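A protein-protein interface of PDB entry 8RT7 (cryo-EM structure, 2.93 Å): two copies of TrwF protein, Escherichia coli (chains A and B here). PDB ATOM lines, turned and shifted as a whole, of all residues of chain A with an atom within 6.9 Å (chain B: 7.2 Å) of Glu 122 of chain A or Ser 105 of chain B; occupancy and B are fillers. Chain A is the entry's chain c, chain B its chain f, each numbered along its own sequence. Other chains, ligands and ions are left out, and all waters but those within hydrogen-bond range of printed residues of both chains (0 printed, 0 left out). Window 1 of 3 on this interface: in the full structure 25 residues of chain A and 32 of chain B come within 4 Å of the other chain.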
ATOM      1  N   PRO A  24     -12.510  10.875  19.632  1.00  0.00           N
ATOM      2  CA  PRO A  24     -11.543  11.941  19.368  1.00  0.00           C
ATOM      3  C   PRO A  24     -10.409  11.921  20.378  1.00  0.00           C
ATOM      4  O   PRO A  24     -10.587  11.543  21.538  1.00  0.00           O
ATOM      5  CB  PRO A  24     -12.380  13.217  19.489  1.00  0.00           C
ATOM      6  CG  PRO A  24     -13.770  12.775  19.191  1.00  0.00           C
ATOM      7  CD  PRO A  24     -13.884  11.390  19.744  1.00  0.00           C
ATOM      8  N   ARG A  32      -9.367  19.455  26.463  1.00  0.00           N
ATOM      9  CA  ARG A  32     -10.642  19.887  25.913  1.00  0.00           C
ATOM     10  C   ARG A  32     -10.627  19.992  24.397  1.00  0.00           C
ATOM     11  O   ARG A  32     -11.692  20.159  23.794  1.00  0.00           O
ATOM     12  CB  ARG A  32     -11.023  21.229  26.531  1.00  0.00           C
ATOM     13  CG  ARG A  32     -11.070  21.194  28.046  1.00  0.00           C
ATOM     14  CD  ARG A  32     -11.169  22.583  28.626  1.00  0.00           C
ATOM     15  NE  ARG A  32     -11.272  22.570  30.080  1.00  0.00           N
ATOM     16  CZ  ARG A  32     -10.228  22.609  30.898  1.00  0.00           C
ATOM     17  NH1 ARG A  32      -9.001  22.660  30.402  1.00  0.00           N
ATOM     18  NH2 ARG A  32     -10.411  22.595  32.210  1.00  0.00           N
ATOM     19  N   ILE A  33      -9.459  19.892  23.772  1.00  0.00           N
ATOM     20  CA  ILE A  33      -9.298  20.071  22.336  1.00  0.00           C
ATOM     21  C   ILE A  33      -8.898  18.727  21.752  1.00  0.00           C
ATOM     22  O   ILE A  33      -7.799  18.228  22.021  1.00  0.00           O
ATOM     23  CB  ILE A  33      -8.255  21.145  22.026  1.00  0.00           C
ATOM     24  CG1 ILE A  33      -8.734  22.479  22.581  1.00  0.00           C
ATOM     25  CG2 ILE A  33      -8.030  21.241  20.535  1.00  0.00           C
ATOM     26  CD1 ILE A  33      -7.698  23.532  22.570  1.00  0.00           C
ATOM     27  N   ARG A  34      -9.777  18.143  20.944  1.00  0.00           N
ATOM     28  CA  ARG A  34      -9.619  16.767  20.504  1.00  0.00           C
ATOM     29  C   ARG A  34      -9.722  16.683  18.989  1.00  0.00           C
ATOM     30  O   ARG A  34     -10.448  17.452  18.357  1.00  0.00           O
ATOM     31  CB  ARG A  34     -10.671  15.869  21.151  1.00  0.00           C
ATOM     32  CG  ARG A  34     -10.615  15.844  22.669  1.00  0.00           C
ATOM     33  CD  ARG A  34     -11.803  15.099  23.228  1.00  0.00           C
ATOM     34  NE  ARG A  34     -11.927  15.234  24.673  1.00  0.00           N
ATOM     35  CZ  ARG A  34     -13.017  14.902  25.353  1.00  0.00           C
ATOM     36  NH1 ARG A  34     -14.076  14.428  24.711  1.00  0.00           N
ATOM     37  NH2 ARG A  34     -13.059  15.052  26.668  1.00  0.00           N
ATOM     38  N   TYR A  35      -8.998  15.723  18.416  1.00  0.00           N
ATOM     39  CA  TYR A  35      -8.909  15.539  16.975  1.00  0.00           C
ATOM     40  C   TYR A  35      -9.467  14.173  16.608  1.00  0.00           C
ATOM     41  O   TYR A  35      -9.294  13.204  17.351  1.00  0.00           O
ATOM     42  CB  TYR A  35      -7.462  15.631  16.486  1.00  0.00           C
ATOM     43  CG  TYR A  35      -6.678  16.792  17.046  1.00  0.00           C
ATOM     44  CD1 TYR A  35      -6.123  16.723  18.314  1.00  0.00           C
ATOM     45  CD2 TYR A  35      -6.480  17.949  16.308  1.00  0.00           C
ATOM     46  CE1 TYR A  35      -5.405  17.772  18.834  1.00  0.00           C
ATOM     47  CE2 TYR A  35      -5.759  19.005  16.824  1.00  0.00           C
ATOM     48  CZ  TYR A  35      -5.225  18.908  18.088  1.00  0.00           C
ATOM     49  OH  TYR A  35      -4.504  19.947  18.620  1.00  0.00           O
ATOM     50  N   ALA A  53     -20.033  24.688  25.341  1.00  0.00           N
ATOM     51  CA  ALA A  53     -20.336  24.698  23.920  1.00  0.00           C
ATOM     52  C   ALA A  53     -19.258  23.922  23.183  1.00  0.00           C
ATOM     53  O   ALA A  53     -18.066  24.193  23.356  1.00  0.00           O
ATOM     54  CB  ALA A  53     -20.423  26.129  23.391  1.00  0.00           C
ATOM     55  N   THR A  54     -19.676  22.956  22.374  1.00  0.00           N
ATOM     56  CA  THR A  54     -18.760  22.168  21.564  1.00  0.00           C
ATOM     57  C   THR A  54     -18.760  22.714  20.145  1.00  0.00           C
ATOM     58  O   THR A  54     -19.826  22.906  19.550  1.00  0.00           O
ATOM     59  CB  THR A  54     -19.152  20.690  21.569  1.00  0.00           C
ATOM     60  OG1 THR A  54     -18.983  20.153  22.885  1.00  0.00           O
ATOM     61  CG2 THR A  54     -18.296  19.903  20.594  1.00  0.00           C
ATOM     62  N   HIS A  55     -17.571  22.969  19.610  1.00  0.00           N
ATOM     63  CA  HIS A  55     -17.415  23.534  18.277  1.00  0.00           C
ATOM     64  C   HIS A  55     -16.978  22.429  17.326  1.00  0.00           C
ATOM     65  O   HIS A  55     -15.865  21.910  17.434  1.00  0.00           O
ATOM     66  CB  HIS A  55     -16.410  24.684  18.298  1.00  0.00           C
ATOM     67  CG  HIS A  55     -16.050  25.202  16.942  1.00  0.00           C
ATOM     68  ND1 HIS A  55     -14.834  25.788  16.669  1.00  0.00           N
ATOM     69  CD2 HIS A  55     -16.748  25.230  15.782  1.00  0.00           C
ATOM     70  CE1 HIS A  55     -14.796  26.153  15.401  1.00  0.00           C
ATOM     71  NE2 HIS A  55     -15.945  25.823  14.840  1.00  0.00           N
ATOM     72  N   ILE A  56     -17.853  22.072  16.395  1.00  0.00           N
ATOM     73  CA  ILE A  56     -17.568  21.060  15.388  1.00  0.00           C
ATOM     74  C   ILE A  56     -17.324  21.782  14.071  1.00  0.00           C
ATOM     75  O   ILE A  56     -18.270  22.187  13.388  1.00  0.00           O
ATOM     76  CB  ILE A  56     -18.710  20.044  15.271  1.00  0.00           C
ATOM     77  CG1 ILE A  56     -18.983  19.402  16.628  1.00  0.00           C
ATOM     78  CG2 ILE A  56     -18.368  18.975  14.254  1.00  0.00           C
ATOM     79  CD1 ILE A  56     -20.165  18.477  16.632  1.00  0.00           C
ATOM     80  N   MET A  57     -16.055  21.939  13.708  1.00  0.00           N
ATOM     81  CA  MET A  57     -15.645  22.705  12.538  1.00  0.00           C
ATOM     82  C   MET A  57     -15.674  21.818  11.302  1.00  0.00           C
ATOM     83  O   MET A  57     -15.122  20.714  11.313  1.00  0.00           O
ATOM     84  CB  MET A  57     -14.245  23.282  12.744  1.00  0.00           C
ATOM     85  CG  MET A  57     -14.005  24.603  12.043  1.00  0.00           C
ATOM     86  SD  MET A  57     -12.713  25.554  12.863  1.00  0.00           S
ATOM     87  CE  MET A  57     -11.365  24.382  12.821  1.00  0.00           C
ATOM     88  N   HIS A  83     -18.871  26.551  10.626  1.00  0.00           N
ATOM     89  CA  HIS A  83     -18.690  26.387  12.060  1.00  0.00           C
ATOM     90  C   HIS A  83     -20.004  25.955  12.690  1.00  0.00           C
ATOM     91  O   HIS A  83     -21.044  26.577  12.454  1.00  0.00           O
ATOM     92  CB  HIS A  83     -18.199  27.688  12.693  1.00  0.00           C
ATOM     93  CG  HIS A  83     -16.887  28.154  12.155  1.00  0.00           C
ATOM     94  ND1 HIS A  83     -15.694  27.546  12.478  1.00  0.00           N
ATOM     95  CD2 HIS A  83     -16.580  29.150  11.292  1.00  0.00           C
ATOM     96  CE1 HIS A  83     -14.706  28.161  11.853  1.00  0.00           C
ATOM     97  NE2 HIS A  83     -15.217  29.137  11.126  1.00  0.00           N
ATOM     98  N   PHE A  85     -21.815  24.822  16.400  1.00  0.00           N
ATOM     99  CA  PHE A  85     -21.768  24.795  17.853  1.00  0.00           C
ATOM    100  C   PHE A  85     -22.960  24.012  18.382  1.00  0.00           C
ATOM    101  O   PHE A  85     -24.064  24.107  17.837  1.00  0.00           O
ATOM    102  CB  PHE A  85     -21.781  26.207  18.439  1.00  0.00           C
ATOM    103  CG  PHE A  85     -20.631  27.057  18.002  1.00  0.00           C
ATOM    104  CD1 PHE A  85     -19.512  27.190  18.798  1.00  0.00           C
ATOM    105  CD2 PHE A  85     -20.666  27.723  16.792  1.00  0.00           C
ATOM    106  CE1 PHE A  85     -18.454  27.979  18.399  1.00  0.00           C
ATOM    107  CE2 PHE A  85     -19.609  28.508  16.388  1.00  0.00           C
ATOM    108  CZ  PHE A  85     -18.504  28.637  17.192  1.00  0.00           C
ATOM    109  N   MET A 120     -15.100  18.930  26.233  1.00  0.00           N
ATOM    110  CA  MET A 120     -14.605  19.078  24.869  1.00  0.00           C
ATOM    111  C   MET A 120     -14.952  20.473  24.382  1.00  0.00           C
ATOM    112  O   MET A 120     -16.119  20.876  24.435  1.00  0.00           O
ATOM    113  CB  MET A 120     -15.219  18.036  23.934  1.00  0.00           C
ATOM    114  CG  MET A 120     -14.415  17.794  22.675  1.00  0.00           C
ATOM    115  SD  MET A 120     -14.767  16.196  21.925  1.00  0.00           S
ATOM    116  CE  MET A 120     -16.444  16.467  21.377  1.00  0.00           C
ATOM    117  N   TYR A 121     -13.955  21.207  23.896  1.00  0.00           N
ATOM    118  CA  TYR A 121     -14.233  22.542  23.382  1.00  0.00           C
ATOM    119  C   TYR A 121     -14.456  22.535  21.872  1.00  0.00           C
ATOM    120  O   TYR A 121     -15.529  22.928  21.403  1.00  0.00           O
ATOM    121  CB  TYR A 121     -13.105  23.497  23.762  1.00  0.00           C
ATOM    122  CG  TYR A 121     -13.230  24.030  25.171  1.00  0.00           C
ATOM    123  CD1 TYR A 121     -13.935  23.327  26.138  1.00  0.00           C
ATOM    124  CD2 TYR A 121     -12.646  25.230  25.535  1.00  0.00           C
ATOM    125  CE1 TYR A 121     -14.057  23.803  27.418  1.00  0.00           C
ATOM    126  CE2 TYR A 121     -12.759  25.712  26.818  1.00  0.00           C
ATOM    127  CZ  TYR A 121     -13.463  24.993  27.756  1.00  0.00           C
ATOM    128  OH  TYR A 121     -13.580  25.471  29.040  1.00  0.00           O
ATOM    129  N   GLU A 122     -13.468  22.085  21.098  1.00  0.00           N
ATOM    130  CA  GLU A 122     -13.639  21.920  19.664  1.00  0.00           C
ATOM    131  C   GLU A 122     -13.363  20.489  19.240  1.00  0.00           C
ATOM    132  O   GLU A 122     -12.600  19.764  19.878  1.00  0.00           O
ATOM    133  CB  GLU A 122     -12.742  22.835  18.832  1.00  0.00           C
ATOM    134  CG  GLU A 122     -13.054  24.302  18.931  1.00  0.00           C
ATOM    135  CD  GLU A 122     -12.122  25.144  18.086  1.00  0.00           C
ATOM    136  OE1 GLU A 122     -11.160  24.581  17.526  1.00  0.00           O
ATOM    137  OE2 GLU A 122     -12.354  26.365  17.979  1.00  0.00           O
ATOM    138  N   LEU A 123     -14.003  20.103  18.144  1.00  0.00           N
ATOM    139  CA  LEU A 123     -13.732  18.856  17.447  1.00  0.00           C
ATOM    140  C   LEU A 123     -13.155  19.192  16.079  1.00  0.00           C
ATOM    141  O   LEU A 123     -13.857  19.743  15.224  1.00  0.00           O
ATOM    142  CB  LEU A 123     -15.005  18.023  17.307  1.00  0.00           C
ATOM    143  CG  LEU A 123     -14.791  16.635  16.716  1.00  0.00           C
ATOM    144  CD1 LEU A 123     -13.658  15.946  17.449  1.00  0.00           C
ATOM    145  CD2 LEU A 123     -16.065  15.817  16.798  1.00  0.00           C
ATOM    146  N   ALA A 124     -11.884  18.860  15.875  1.00  0.00           N
ATOM    147  CA  ALA A 124     -11.191  19.122  14.624  1.00  0.00           C
ATOM    148  C   ALA A 124     -10.958  17.810  13.893  1.00  0.00           C
ATOM    149  O   ALA A 124     -10.623  16.796  14.510  1.00  0.00           O
ATOM    150  CB  ALA A 124      -9.863  19.838  14.866  1.00  0.00           C
ATOM    151  N   TYR B  38      -0.941  33.209  21.981  1.00  0.00           N
ATOM    152  CA  TYR B  38      -1.954  32.364  21.374  1.00  0.00           C
ATOM    153  C   TYR B  38      -1.401  30.973  21.097  1.00  0.00           C
ATOM    154  O   TYR B  38      -0.190  30.767  20.992  1.00  0.00           O
ATOM    155  CB  TYR B  38      -2.465  32.992  20.079  1.00  0.00           C
ATOM    156  CG  TYR B  38      -3.633  32.265  19.457  1.00  0.00           C
ATOM    157  CD1 TYR B  38      -4.928  32.509  19.878  1.00  0.00           C
ATOM    158  CD2 TYR B  38      -3.442  31.340  18.446  1.00  0.00           C
ATOM    159  CE1 TYR B  38      -5.996  31.851  19.314  1.00  0.00           C
ATOM    160  CE2 TYR B  38      -4.504  30.677  17.877  1.00  0.00           C
ATOM    161  CZ  TYR B  38      -5.779  30.937  18.315  1.00  0.00           C
ATOM    162  OH  TYR B  38      -6.843  30.277  17.749  1.00  0.00           O
ATOM    163  N   ASN B  39      -2.305  30.014  20.997  1.00  0.00           N
ATOM    164  CA  ASN B  39      -1.999  28.639  20.641  1.00  0.00           C
ATOM    165  C   ASN B  39      -3.297  27.992  20.182  1.00  0.00           C
ATOM    166  O   ASN B  39      -4.304  28.061  20.897  1.00  0.00           O
ATOM    167  CB  ASN B  39      -1.394  27.892  21.830  1.00  0.00           C
ATOM    168  CG  ASN B  39      -0.726  26.593  21.429  1.00  0.00           C
ATOM    169  OD1 ASN B  39      -1.146  25.514  21.840  1.00  0.00           O
ATOM    170  ND2 ASN B  39       0.330  26.691  20.633  1.00  0.00           N
ATOM    171  N   PRO B  40      -3.329  27.363  19.009  1.00  0.00           N
ATOM    172  CA  PRO B  40      -4.608  26.854  18.499  1.00  0.00           C
ATOM    173  C   PRO B  40      -5.050  25.561  19.151  1.00  0.00           C
ATOM    174  O   PRO B  40      -6.164  25.099  18.879  1.00  0.00           O
ATOM    175  CB  PRO B  40      -4.331  26.671  17.003  1.00  0.00           C
ATOM    176  CG  PRO B  40      -2.818  26.449  16.916  1.00  0.00           C
ATOM    177  CD  PRO B  40      -2.199  26.786  18.265  1.00  0.00           C
ATOM    178  N   ASP B  42      -4.753  25.053  22.690  1.00  0.00           N
ATOM    179  CA  ASP B  42      -4.813  25.274  24.127  1.00  0.00           C
ATOM    180  C   ASP B  42      -5.840  26.355  24.424  1.00  0.00           C
ATOM    181  O   ASP B  42      -6.145  27.199  23.579  1.00  0.00           O
ATOM    182  CB  ASP B  42      -3.443  25.662  24.693  1.00  0.00           C
ATOM    183  CG  ASP B  42      -3.354  25.452  26.190  1.00  0.00           C
ATOM    184  OD1 ASP B  42      -4.396  25.175  26.819  1.00  0.00           O
ATOM    185  OD2 ASP B  42      -2.235  25.544  26.738  1.00  0.00           O
ATOM    186  N   GLU B  62      -8.486  41.560  12.167  1.00  0.00           N
ATOM    187  CA  GLU B  62      -9.176  40.309  12.441  1.00  0.00           C
ATOM    188  C   GLU B  62     -10.679  40.520  12.356  1.00  0.00           C
ATOM    189  O   GLU B  62     -11.228  41.413  13.009  1.00  0.00           O
ATOM    190  CB  GLU B  62      -8.794  39.783  13.820  1.00  0.00           C
ATOM    191  CG  GLU B  62      -9.437  38.468  14.165  1.00  0.00           C
ATOM    192  CD  GLU B  62      -8.514  37.570  14.946  1.00  0.00           C
ATOM    193  OE1 GLU B  62      -7.591  38.095  15.600  1.00  0.00           O
ATOM    194  OE2 GLU B  62      -8.704  36.339  14.903  1.00  0.00           O
ATOM    195  N   ASN B  96     -17.599  28.120  29.302  1.00  0.00           N
ATOM    196  CA  ASN B  96     -16.553  28.261  28.304  1.00  0.00           C
ATOM    197  C   ASN B  96     -16.970  29.275  27.249  1.00  0.00           C
ATOM    198  O   ASN B  96     -18.153  29.421  26.933  1.00  0.00           O
ATOM    199  CB  ASN B  96     -16.224  26.914  27.640  1.00  0.00           C
ATOM    200  CG  ASN B  96     -17.319  26.426  26.707  1.00  0.00           C
ATOM    201  OD1 ASN B  96     -18.498  26.690  26.918  1.00  0.00           O
ATOM    202  ND2 ASN B  96     -16.925  25.691  25.673  1.00  0.00           N
ATOM    203  N   ILE B  98     -16.023  30.434  23.266  1.00  0.00           N
ATOM    204  CA  ILE B  98     -15.377  30.101  22.004  1.00  0.00           C
ATOM    205  C   ILE B  98     -15.827  31.147  20.996  1.00  0.00           C
ATOM    206  O   ILE B  98     -16.971  31.121  20.531  1.00  0.00           O
ATOM    207  CB  ILE B  98     -15.712  28.688  21.523  1.00  0.00           C
ATOM    208  CG1 ILE B  98     -15.189  27.653  22.517  1.00  0.00           C
ATOM    209  CG2 ILE B  98     -15.139  28.451  20.143  1.00  0.00           C
ATOM    210  CD1 ILE B  98     -15.689  26.257  22.266  1.00  0.00           C
ATOM    211  N   VAL B  99     -14.933  32.070  20.656  1.00  0.00           N
ATOM    212  CA  VAL B  99     -15.199  33.104  19.664  1.00  0.00           C
ATOM    213  C   VAL B  99     -14.383  32.786  18.418  1.00  0.00           C
ATOM    214  O   VAL B  99     -13.158  32.630  18.484  1.00  0.00           O
ATOM    215  CB  VAL B  99     -14.906  34.510  20.220  1.00  0.00           C
ATOM    216  CG1 VAL B  99     -13.444  34.701  20.547  1.00  0.00           C
ATOM    217  CG2 VAL B  99     -15.346  35.561  19.227  1.00  0.00           C
ATOM    218  N   VAL B 100     -15.068  32.637  17.289  1.00  0.00           N
ATOM    219  CA  VAL B 100     -14.421  32.322  16.022  1.00  0.00           C
ATOM    220  C   VAL B 100     -14.278  33.603  15.221  1.00  0.00           C
ATOM    221  O   VAL B 100     -15.134  34.493  15.284  1.00  0.00           O
ATOM    222  CB  VAL B 100     -15.198  31.256  15.227  1.00  0.00           C
ATOM    223  CG1 VAL B 100     -15.255  29.957  16.001  1.00  0.00           C
ATOM    224  CG2 VAL B 100     -16.588  31.742  14.890  1.00  0.00           C
ATOM    225  N   THR B 101     -13.184  33.708  14.482  1.00  0.00           N
ATOM    226  CA  THR B 101     -12.892  34.875  13.672  1.00  0.00           C
ATOM    227  C   THR B 101     -12.485  34.423  12.278  1.00  0.00           C
ATOM    228  O   THR B 101     -12.386  33.226  11.991  1.00  0.00           O
ATOM    229  CB  THR B 101     -11.791  35.731  14.307  1.00  0.00           C
ATOM    230  OG1 THR B 101     -10.705  34.890  14.709  1.00  0.00           O
ATOM    231  CG2 THR B 101     -12.324  36.471  15.517  1.00  0.00           C
ATOM    232  N   ASP B 102     -12.252  35.404  11.408  1.00  0.00           N
ATOM    233  CA  ASP B 102     -11.859  35.108  10.036  1.00  0.00           C
ATOM    234  C   ASP B 102     -10.541  34.346  10.019  1.00  0.00           C
ATOM    235  O   ASP B 102     -10.402  33.340   9.314  1.00  0.00           O
ATOM    236  CB  ASP B 102     -11.781  36.432   9.260  1.00  0.00           C
ATOM    237  CG  ASP B 102     -11.056  36.343   7.917  1.00  0.00           C
ATOM    238  OD1 ASP B 102     -11.085  37.367   7.205  1.00  0.00           O
ATOM    239  OD2 ASP B 102     -10.510  35.295   7.523  1.00  0.00           O
ATOM    240  N   ARG B 103      -9.581  34.783  10.827  1.00  0.00           N
ATOM    241  CA  ARG B 103      -8.254  34.186  10.806  1.00  0.00           C
ATOM    242  C   ARG B 103      -8.191  32.939  11.679  1.00  0.00           C
ATOM    243  O   ARG B 103      -7.900  31.843  11.189  1.00  0.00           O
ATOM    244  CB  ARG B 103      -7.230  35.224  11.261  1.00  0.00           C
ATOM    245  CG  ARG B 103      -5.783  34.839  11.051  1.00  0.00           C
ATOM    246  CD  ARG B 103      -4.889  36.024  11.353  1.00  0.00           C
ATOM    247  NE  ARG B 103      -5.139  37.141  10.442  1.00  0.00           N
ATOM    248  CZ  ARG B 103      -5.677  38.299  10.811  1.00  0.00           C
ATOM    249  NH1 ARG B 103      -6.024  38.495  12.073  1.00  0.00           N
ATOM    250  NH2 ARG B 103      -5.866  39.262   9.921  1.00  0.00           N
ATOM    251  N   ARG B 104      -8.477  33.086  12.970  1.00  0.00           N
ATOM    252  CA  ARG B 104      -8.368  31.987  13.919  1.00  0.00           C
ATOM    253  C   ARG B 104      -9.644  31.834  14.735  1.00  0.00           C
ATOM    254  O   ARG B 104     -10.663  32.461  14.429  1.00  0.00           O
ATOM    255  CB  ARG B 104      -7.179  32.215  14.845  1.00  0.00           C
ATOM    256  CG  ARG B 104      -7.187  33.573  15.501  1.00  0.00           C
ATOM    257  CD  ARG B 104      -5.965  33.770  16.365  1.00  0.00           C
ATOM    258  NE  ARG B 104      -4.837  34.295  15.605  1.00  0.00           N
ATOM    259  CZ  ARG B 104      -4.617  35.586  15.389  1.00  0.00           C
ATOM    260  NH1 ARG B 104      -5.442  36.497  15.881  1.00  0.00           N
ATOM    261  NH2 ARG B 104      -3.565  35.967  14.687  1.00  0.00           N
ATOM    262  N   SER B 105      -9.597  30.999  15.771  1.00  0.00           N
ATOM    263  CA  SER B 105     -10.717  30.813  16.685  1.00  0.00           C
ATOM    264  C   SER B 105     -10.184  30.659  18.100  1.00  0.00           C
ATOM    265  O   SER B 105      -9.378  29.763  18.366  1.00  0.00           O
ATOM    266  CB  SER B 105     -11.549  29.589  16.302  1.00  0.00           C
ATOM    267  OG  SER B 105     -12.379  29.196  17.378  1.00  0.00           O
ATOM    268  N   TYR B 106     -10.634  31.527  18.998  1.00  0.00           N
ATOM    269  CA  TYR B 106     -10.156  31.544  20.371  1.00  0.00           C
ATOM    270  C   TYR B 106     -10.938  30.561  21.236  1.00  0.00           C
ATOM    271  O   TYR B 106     -11.962  30.007  20.830  1.00  0.00           O
ATOM    272  CB  TYR B 106     -10.261  32.949  20.951  1.00  0.00           C
ATOM    273  CG  TYR B 106      -9.406  33.976  20.259  1.00  0.00           C
ATOM    274  CD1 TYR B 106      -8.213  34.402  20.818  1.00  0.00           C
ATOM    275  CD2 TYR B 106      -9.791  34.520  19.044  1.00  0.00           C
ATOM    276  CE1 TYR B 106      -7.433  35.341  20.192  1.00  0.00           C
ATOM    277  CE2 TYR B 106      -9.017  35.458  18.409  1.00  0.00           C
ATOM    278  CZ  TYR B 106      -7.840  35.866  18.985  1.00  0.00           C
ATOM    279  OH  TYR B 106      -7.067  36.803  18.345  1.00  0.00           O
ATOM    280  N   LYS B 107     -10.447  30.361  22.459  1.00  0.00           N
ATOM    281  CA  LYS B 107     -11.014  29.386  23.386  1.00  0.00           C
ATOM    282  C   LYS B 107     -10.762  29.893  24.793  1.00  0.00           C
ATOM    283  O   LYS B 107      -9.605  30.087  25.173  1.00  0.00           O
ATOM    284  CB  LYS B 107     -10.360  28.026  23.214  1.00  0.00           C
ATOM    285  CG  LYS B 107     -10.605  27.359  21.901  1.00  0.00           C
ATOM    286  CD  LYS B 107      -9.903  26.040  21.900  1.00  0.00           C
ATOM    287  CE  LYS B 107     -10.172  25.284  20.640  1.00  0.00           C
ATOM    288  NZ  LYS B 107      -9.551  25.996  19.485  1.00  0.00           N
ATOM    289  N   PHE B 108     -11.819  30.091  25.569  1.00  0.00           N
ATOM    290  CA  PHE B 108     -11.676  30.656  26.900  1.00  0.00           C
ATOM    291  C   PHE B 108     -12.310  29.725  27.922  1.00  0.00           C
ATOM    292  O   PHE B 108     -13.264  29.004  27.620  1.00  0.00           O
ATOM    293  CB  PHE B 108     -12.324  32.045  27.002  1.00  0.00           C
ATOM    294  CG  PHE B 108     -11.654  33.103  26.169  1.00  0.00           C
ATOM    295  CD1 PHE B 108     -11.108  34.220  26.760  1.00  0.00           C
ATOM    296  CD2 PHE B 108     -11.636  33.018  24.793  1.00  0.00           C
ATOM    297  CE1 PHE B 108     -10.508  35.202  26.001  1.00  0.00           C
ATOM    298  CE2 PHE B 108     -11.043  34.000  24.035  1.00  0.00           C
ATOM    299  CZ  PHE B 108     -10.479  35.090  24.637  1.00  0.00           C
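Asp 42 of chain B touches Ile 33 of chain A. CD of Lys 107 of chain B touches CD1 of Ile 33 of chain A, 3.4 Å away. Ala 53 of chain A touches Ile 98 of chain B (O to CD1, 3.3 Å). His 55 of chain A touches Val 100 of chain B. CE1 of Phe 85 of chain A touches CG2 of Ile 98 of chain B, at 3.8 Å. CG1 of Val 100 of chain B touches CZ of Phe 85 of chain A, 3.7 Å away. Tyr 121 of chain A touches Asn 96 of chain B (OH to CB, 3.3 Å). CD1 of Ile 98 of chain B touches O of Tyr 121 of chain A, at 3.4 Å. O of Phe 108 of chain B touches CE2 of Tyr 121 of chain A (3.4 Å).
Of the 17 printed residues of chain B, 7 touch a printed residue of chain A. Hydrophobic or aromatic side chains of chain B within 4 Å of the printed part of chain A: Ile 98 and Val 100. Among the printed residues, Asp or Glu carboxylates within 4 Å of a Lys or Arg side-chain nitrogen of the other chain: Glu 122 of chain A with Lys 107 of chain B (2.9 Å).
The backbone NH of Tyr 121 of chain A sits at hydrogen-bond distance from the backbone carbonyl oxygen of Arg 32 of chain A (2.5 Å). A ring nitrogen (NE2) of His 55 of chain A sits close to the side-chain sulfur (SD) of Met 57 of chain A. A ring nitrogen (ND1) of His 83 of chain A sits at hydrogen-bond distance from a ring nitrogen (NE2) of His 55 of chain A, 2.9 Å away. The backbone carbonyl oxygen of Tyr 121 of chain A sits at hydrogen-bond distance from the backbone NH of His 55 of chain A (2.7 Å). A ring nitrogen (ND1) of His 55 of chain A sits at hydrogen-bond distance from the side-chain carboxylate (OE2) of Glu 122 of chain A. The backbone carbonyl oxygen (O) of His 55 of chain A lies within hydrogen-bond range of the backbone NH (N) of Leu 123 of chain A (2.7 Å).
No position is printed for both chains.
Glu 122 of chain A touches just these residues of chain B: Ser 105 (2.9 Å) and Lys 107 (2.9 Å). Ser 105 of chain B touches one residue of chain A. Of the printed residues of chain A, Lys 107 of chain B touches Ile 33 (3.4 Å) and Glu 122 (2.9 Å). Printed residues of chain A within 4 Å of Val 100 of chain B: His 55 (3.9 Å) and Phe 85 (3.7 Å). Of the printed residues of chain B, His 55 of chain A touches Val 100 (3.9 Å). Pro 24 of chain A touches none of the printed residues of chain B. Met 57 of chain A touches none of the printed residues of chain B. The nearest residue of chain B that does not touch Glu 122 of chain A is Ile 98 of chain B (4.1 Å). The nearest printed residue of chain A that does not touch Val 100 of chain B is His 83 of chain A (4.3 Å).
N of Ala 53 of chain A is in hydrogen-bond range of OD1 of Asn 96 of chain B, at 3.0 Å. The side-chain carboxylate (OE2) of Glu 122 of chain A is in hydrogen-bond range of the side-chain hydroxyl (OG) of Ser 105 of chain B, at 2.9 Å. The side-chain carboxylate (OE1) of Glu 122 of chain A is in salt-bridge range of the side-chain amino group (NZ) of Lys 107 of chain B (2.9 Å).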
